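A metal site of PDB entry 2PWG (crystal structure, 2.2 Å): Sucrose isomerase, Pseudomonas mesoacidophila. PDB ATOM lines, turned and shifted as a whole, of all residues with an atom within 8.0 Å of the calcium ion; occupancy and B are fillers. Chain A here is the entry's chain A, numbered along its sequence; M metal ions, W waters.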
ATOM      1  N   PRO A  16      11.371  25.208 -11.120  1.00  0.00           N
ATOM      2  CA  PRO A  16      11.681  23.991 -10.360  1.00  0.00           C
ATOM      3  C   PRO A  16      12.301  22.847 -11.148  1.00  0.00           C
ATOM      4  O   PRO A  16      13.266  22.233 -10.707  1.00  0.00           O
ATOM      5  CB  PRO A  16      10.344  23.624  -9.727  1.00  0.00           C
ATOM      6  CG  PRO A  16       9.647  24.904  -9.620  1.00  0.00           C
ATOM      7  CD  PRO A  16       9.938  25.528 -10.961  1.00  0.00           C
ATOM      8  N   ARG A  17      11.735  22.574 -12.315  1.00  0.00           N
ATOM      9  CA  ARG A  17      12.203  21.493 -13.139  1.00  0.00           C
ATOM     10  C   ARG A  17      13.713  21.560 -13.382  1.00  0.00           C
ATOM     11  O   ARG A  17      14.368  20.528 -13.532  1.00  0.00           O
ATOM     12  CB  ARG A  17      11.464  21.530 -14.469  1.00  0.00           C
ATOM     13  CG  ARG A  17      11.689  20.343 -15.355  1.00  0.00           C
ATOM     14  CD  ARG A  17      10.994  20.514 -16.702  1.00  0.00           C
ATOM     15  NE  ARG A  17      11.188  19.309 -17.496  1.00  0.00           N
ATOM     16  CZ  ARG A  17      10.428  18.227 -17.390  1.00  0.00           C
ATOM     17  NH1 ARG A  17       9.409  18.204 -16.524  1.00  0.00           N
ATOM     18  NH2 ARG A  17      10.702  17.146 -18.127  1.00  0.00           N
ATOM     19  N   LYS A  20      17.031  22.307  -8.850  1.00  0.00           N
ATOM     20  CA  LYS A  20      17.839  21.385  -8.054  1.00  0.00           C
ATOM     21  C   LYS A  20      17.173  20.025  -7.901  1.00  0.00           C
ATOM     22  O   LYS A  20      16.071  19.916  -7.352  1.00  0.00           O
ATOM     23  CB  LYS A  20      18.111  21.982  -6.667  1.00  0.00           C
ATOM     24  CG  LYS A  20      19.041  21.137  -5.800  1.00  0.00           C
ATOM     25  CD  LYS A  20      20.457  21.153  -6.336  1.00  0.00           C
ATOM     26  CE  LYS A  20      21.190  19.817  -6.094  1.00  0.00           C
ATOM     27  NZ  LYS A  20      21.450  19.483  -4.670  1.00  0.00           N
ATOM     28  N   ASP A  21      17.854  18.988  -8.404  1.00  0.00           N
ATOM     29  CA  ASP A  21      17.384  17.609  -8.316  1.00  0.00           C
ATOM     30  C   ASP A  21      17.980  17.021  -7.039  1.00  0.00           C
ATOM     31  O   ASP A  21      19.186  17.174  -6.790  1.00  0.00           O
ATOM     32  CB  ASP A  21      17.858  16.778  -9.528  1.00  0.00           C
ATOM     33  CG  ASP A  21      17.334  15.341  -9.516  1.00  0.00           C
ATOM     34  OD1 ASP A  21      16.425  15.039  -8.707  1.00  0.00           O
ATOM     35  OD2 ASP A  21      17.800  14.517 -10.323  1.00  0.00           O
ATOM     36  N   THR A  22      17.152  16.380  -6.228  1.00  0.00           N
ATOM     37  CA  THR A  22      17.627  15.790  -4.980  1.00  0.00           C
ATOM     38  C   THR A  22      17.477  14.283  -4.923  1.00  0.00           C
ATOM     39  O   THR A  22      17.869  13.672  -3.948  1.00  0.00           O
ATOM     40  CB  THR A  22      16.884  16.383  -3.760  1.00  0.00           C
ATOM     41  OG1 THR A  22      15.468  16.320  -3.981  1.00  0.00           O
ATOM     42  CG2 THR A  22      17.302  17.820  -3.522  1.00  0.00           C
ATOM     43  N   ASN A  23      16.909  13.665  -5.963  1.00  0.00           N
ATOM     44  CA  ASN A  23      16.708  12.224  -5.952  1.00  0.00           C
ATOM     45  C   ASN A  23      17.226  11.502  -7.223  1.00  0.00           C
ATOM     46  O   ASN A  23      16.825  10.374  -7.497  1.00  0.00           O
ATOM     47  CB  ASN A  23      15.222  11.924  -5.770  1.00  0.00           C
ATOM     48  CG  ASN A  23      14.435  12.243  -7.003  1.00  0.00           C
ATOM     49  OD1 ASN A  23      14.857  13.075  -7.822  1.00  0.00           O
ATOM     50  ND2 ASN A  23      13.287  11.609  -7.172  1.00  0.00           N
ATOM     51  N   GLY A  24      18.058  12.175  -8.009  1.00  0.00           N
ATOM     52  CA  GLY A  24      18.655  11.580  -9.195  1.00  0.00           C
ATOM     53  C   GLY A  24      17.852  11.228 -10.440  1.00  0.00           C
ATOM     54  O   GLY A  24      18.401  10.604 -11.348  1.00  0.00           O
ATOM     55  N   ASP A  25      16.581  11.603 -10.497  1.00  0.00           N
ATOM     56  CA  ASP A  25      15.809  11.292 -11.687  1.00  0.00           C
ATOM     57  C   ASP A  25      16.087  12.284 -12.809  1.00  0.00           C
ATOM     58  O   ASP A  25      15.556  12.163 -13.918  1.00  0.00           O
ATOM     59  CB  ASP A  25      14.318  11.290 -11.364  1.00  0.00           C
ATOM     60  CG  ASP A  25      13.777  12.683 -11.066  1.00  0.00           C
ATOM     61  OD1 ASP A  25      14.564  13.606 -10.741  1.00  0.00           O
ATOM     62  OD2 ASP A  25      12.551  12.832 -11.162  1.00  0.00           O
ATOM     63  N   GLY A  26      16.913  13.289 -12.525  1.00  0.00           N
ATOM     64  CA  GLY A  26      17.230  14.263 -13.550  1.00  0.00           C
ATOM     65  C   GLY A  26      16.341  15.493 -13.570  1.00  0.00           C
ATOM     66  O   GLY A  26      16.588  16.419 -14.353  1.00  0.00           O
ATOM     67  N   ILE A  27      15.311  15.520 -12.731  1.00  0.00           N
ATOM     68  CA  ILE A  27      14.391  16.679 -12.689  1.00  0.00           C
ATOM     69  C   ILE A  27      14.454  17.430 -11.351  1.00  0.00           C
ATOM     70  O   ILE A  27      14.547  16.827 -10.288  1.00  0.00           O
ATOM     71  CB  ILE A  27      12.950  16.216 -12.979  1.00  0.00           C
ATOM     72  CG1 ILE A  27      12.883  15.741 -14.430  1.00  0.00           C
ATOM     73  CG2 ILE A  27      11.948  17.341 -12.682  1.00  0.00           C
ATOM     74  CD1 ILE A  27      11.717  14.844 -14.731  1.00  0.00           C
ATOM     75  N   GLY A  28      14.440  18.761 -11.407  1.00  0.00           N
ATOM     76  CA  GLY A  28      14.492  19.525 -10.177  1.00  0.00           C
ATOM     77  C   GLY A  28      13.241  19.241  -9.363  1.00  0.00           C
ATOM     78  O   GLY A  28      12.209  18.829  -9.911  1.00  0.00           O
ATOM     79  N   ASP A  29      13.319  19.457  -8.056  1.00  0.00           N
ATOM     80  CA  ASP A  29      12.167  19.180  -7.208  1.00  0.00           C
ATOM     81  C   ASP A  29      12.079  20.128  -6.005  1.00  0.00           C
ATOM     82  O   ASP A  29      12.962  20.963  -5.807  1.00  0.00           O
ATOM     83  CB  ASP A  29      12.269  17.738  -6.744  1.00  0.00           C
ATOM     84  CG  ASP A  29      13.670  17.375  -6.310  1.00  0.00           C
ATOM     85  OD1 ASP A  29      14.198  18.011  -5.366  1.00  0.00           O
ATOM     86  OD2 ASP A  29      14.257  16.456  -6.923  1.00  0.00           O
ATOM     87  N   PHE A  30      11.000  19.995  -5.238  1.00  0.00           N
ATOM     88  CA  PHE A  30      10.782  20.840  -4.061  1.00  0.00           C
ATOM     89  C   PHE A  30      11.887  20.745  -3.024  1.00  0.00           C
ATOM     90  O   PHE A  30      12.308  21.771  -2.482  1.00  0.00           O
ATOM     91  CB  PHE A  30       9.472  20.494  -3.372  1.00  0.00           C
ATOM     92  CG  PHE A  30       8.263  20.918  -4.129  1.00  0.00           C
ATOM     93  CD1 PHE A  30       8.117  22.240  -4.547  1.00  0.00           C
ATOM     94  CD2 PHE A  30       7.252  20.018  -4.391  1.00  0.00           C
ATOM     95  CE1 PHE A  30       6.966  22.661  -5.221  1.00  0.00           C
ATOM     96  CE2 PHE A  30       6.107  20.428  -5.071  1.00  0.00           C
ATOM     97  CZ  PHE A  30       5.959  21.751  -5.476  1.00  0.00           C
ATOM     98  N   LYS A  31      12.325  19.526  -2.719  1.00  0.00           N
ATOM     99  CA  LYS A  31      13.397  19.381  -1.736  1.00  0.00           C
ATOM    100  C   LYS A  31      14.633  20.125  -2.206  1.00  0.00           C
ATOM    101  O   LYS A  31      15.357  20.716  -1.395  1.00  0.00           O
ATOM    102  CB  LYS A  31      13.733  17.909  -1.490  1.00  0.00           C
ATOM    103  CG  LYS A  31      12.615  17.142  -0.818  1.00  0.00           C
ATOM    104  CD  LYS A  31      13.106  15.818  -0.222  1.00  0.00           C
ATOM    105  CE  LYS A  31      11.963  15.088   0.473  1.00  0.00           C
ATOM    106  NZ  LYS A  31      12.427  14.014   1.413  1.00  0.00           N
ATOM    107  N   GLY A  32      14.874  20.109  -3.514  1.00  0.00           N
ATOM    108  CA  GLY A  32      16.023  20.824  -4.028  1.00  0.00           C
ATOM    109  C   GLY A  32      15.895  22.316  -3.766  1.00  0.00           C
ATOM    110  O   GLY A  32      16.861  22.973  -3.346  1.00  0.00           O
ATOM    111  N   LYS A  73       3.887  15.298  -9.482  1.00  0.00           N
ATOM    112  CA  LYS A  73       4.582  14.101  -9.014  1.00  0.00           C
ATOM    113  C   LYS A  73       6.106  14.265  -9.053  1.00  0.00           C
ATOM    114  O   LYS A  73       6.818  13.871  -8.116  1.00  0.00           O
ATOM    115  CB  LYS A  73       4.143  12.908  -9.868  1.00  0.00           C
ATOM    116  CG  LYS A  73       4.543  11.534  -9.315  1.00  0.00           C
ATOM    117  CD  LYS A  73       3.973  10.373 -10.173  1.00  0.00           C
ATOM    118  CE  LYS A  73       4.176   8.995  -9.489  1.00  0.00           C
ATOM    119  NZ  LYS A  73       3.657   7.820 -10.285  1.00  0.00           N
ATOM    120  N   GLU A  74       6.626  14.875 -10.115  1.00  0.00           N
ATOM    121  CA  GLU A  74       8.060  15.068 -10.233  1.00  0.00           C
ATOM    122  C   GLU A  74       8.622  16.015  -9.169  1.00  0.00           C
ATOM    123  O   GLU A  74       9.805  15.907  -8.795  1.00  0.00           O
ATOM    124  CB  GLU A  74       8.444  15.621 -11.618  1.00  0.00           C
ATOM    125  CG  GLU A  74       8.405  14.628 -12.766  1.00  0.00           C
ATOM    126  CD  GLU A  74       6.988  14.240 -13.205  1.00  0.00           C
ATOM    127  OE1 GLU A  74       6.024  14.939 -12.820  1.00  0.00           O
ATOM    128  OE2 GLU A  74       6.861  13.248 -13.946  1.00  0.00           O
ATOM    129  N   TYR A  75       7.805  16.951  -8.685  1.00  0.00           N
ATOM    130  CA  TYR A  75       8.355  17.872  -7.705  1.00  0.00           C
ATOM    131  C   TYR A  75       8.322  17.386  -6.263  1.00  0.00           C
ATOM    132  O   TYR A  75       9.060  17.895  -5.429  1.00  0.00           O
ATOM    133  CB  TYR A  75       7.696  19.238  -7.810  1.00  0.00           C
ATOM    134  CG  TYR A  75       7.948  19.890  -9.142  1.00  0.00           C
ATOM    135  CD1 TYR A  75       9.022  19.492  -9.949  1.00  0.00           C
ATOM    136  CD2 TYR A  75       7.111  20.876  -9.619  1.00  0.00           C
ATOM    137  CE1 TYR A  75       9.231  20.058 -11.182  1.00  0.00           C
ATOM    138  CE2 TYR A  75       7.323  21.464 -10.839  1.00  0.00           C
ATOM    139  CZ  TYR A  75       8.379  21.049 -11.631  1.00  0.00           C
ATOM    140  OH  TYR A  75       8.545  21.611 -12.881  1.00  0.00           O
ATOM    141  N   GLY A  76       7.478  16.394  -5.987  1.00  0.00           N
ATOM    142  CA  GLY A  76       7.392  15.848  -4.634  1.00  0.00           C
ATOM    143  C   GLY A  76       5.971  15.592  -4.175  1.00  0.00           C
ATOM    144  O   GLY A  76       5.121  15.168  -4.960  1.00  0.00           O
ATOM    145  N   PHE A 430      23.780  19.831 -10.317  1.00  0.00           N
ATOM    146  CA  PHE A 430      22.322  19.929 -10.401  1.00  0.00           C
ATOM    147  C   PHE A 430      21.676  18.564 -10.054  1.00  0.00           C
ATOM    148  O   PHE A 430      20.631  18.495  -9.405  1.00  0.00           O
ATOM    149  CB  PHE A 430      21.902  20.341 -11.827  1.00  0.00           C
ATOM    150  CG  PHE A 430      20.433  20.033 -12.162  1.00  0.00           C
ATOM    151  CD1 PHE A 430      19.394  20.735 -11.541  1.00  0.00           C
ATOM    152  CD2 PHE A 430      20.108  19.030 -13.064  1.00  0.00           C
ATOM    153  CE1 PHE A 430      18.059  20.438 -11.819  1.00  0.00           C
ATOM    154  CE2 PHE A 430      18.774  18.732 -13.357  1.00  0.00           C
ATOM    155  CZ  PHE A 430      17.756  19.430 -12.740  1.00  0.00           C
ATOM    156  N   THR A 431      22.322  17.477 -10.490  1.00  0.00           N
ATOM    157  CA  THR A 431      21.799  16.140 -10.273  1.00  0.00           C
ATOM    158  C   THR A 431      22.902  15.104 -10.189  1.00  0.00           C
ATOM    159  O   THR A 431      24.029  15.329 -10.634  1.00  0.00           O
ATOM    160  CB  THR A 431      20.831  15.743 -11.431  1.00  0.00           C
ATOM    161  OG1 THR A 431      20.257  14.469 -11.167  1.00  0.00           O
ATOM    162  CG2 THR A 431      21.588  15.668 -12.752  1.00  0.00           C
HETATM  163 CA    CA M   1      14.064  15.069  -8.782  1.00  0.00          CA
HETATM  164  O   HOH W   1      12.050  14.430  -7.593  1.00  0.00           O
HETATM  165  O   HOH W   2      12.014  14.803  -9.975  1.00  0.00           O
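The backbone carbonyl oxygen (O) of Phe 430 lies within hydrogen-bond range of the backbone NH (N) of Asp 21, 3.0 Å away. The side-chain carboxylate (OD2) of Asp 21 is in hydrogen-bond range of the backbone NH (N) of Gly 26 (2.7 Å). The side-chain carboxylate (OD1) of Asp 29 lies within hydrogen-bond range of the side-chain hydroxyl (OG1) of Thr 22 (2.5 Å). OD2 of Asp 21 sits close to N of Gly 24, 3.3 Å away. The side-chain carboxylate of Asp 21 lies within hydrogen-bond range of the side-chain hydroxyl of Thr 431, 2.6 Å away. The backbone NH (N) of Gly 32 lies within hydrogen-bond range of the side-chain carboxylate (OD1) of Asp 29, 2.9 Å away. The backbone carbonyl oxygen of Lys 20 lies within hydrogen-bond range of the backbone NH of Asp 29, 2.9 Å away.
Within 4 Å of the calcium ion: Asp 21, Asn 23, Asp 25, Ile 27 and Asp 29. The nearest printed residue that does not touch the calcium ion is Thr 22 (4.2 Å).
The calcium ion is bound by OD2 of Asp 29 (2.3 Å), OD1 of Asn 23 (2.4 Å), OD1 of Asp 21 (2.4 Å), O of Ile 27 (2.4 Å), water W2 (2.4 Å), water W1 (2.4 Å) and OD1 of Asp 25 (2.5 Å). The calcium ion has seven donor atoms within binding distance.
Water W1 lies within hydrogen-bond range of the backbone carbonyl oxygen (O) of Glu 74 (2.9 Å) and the side-chain amide nitrogen (ND2) of Asn 23 (3.1 Å).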
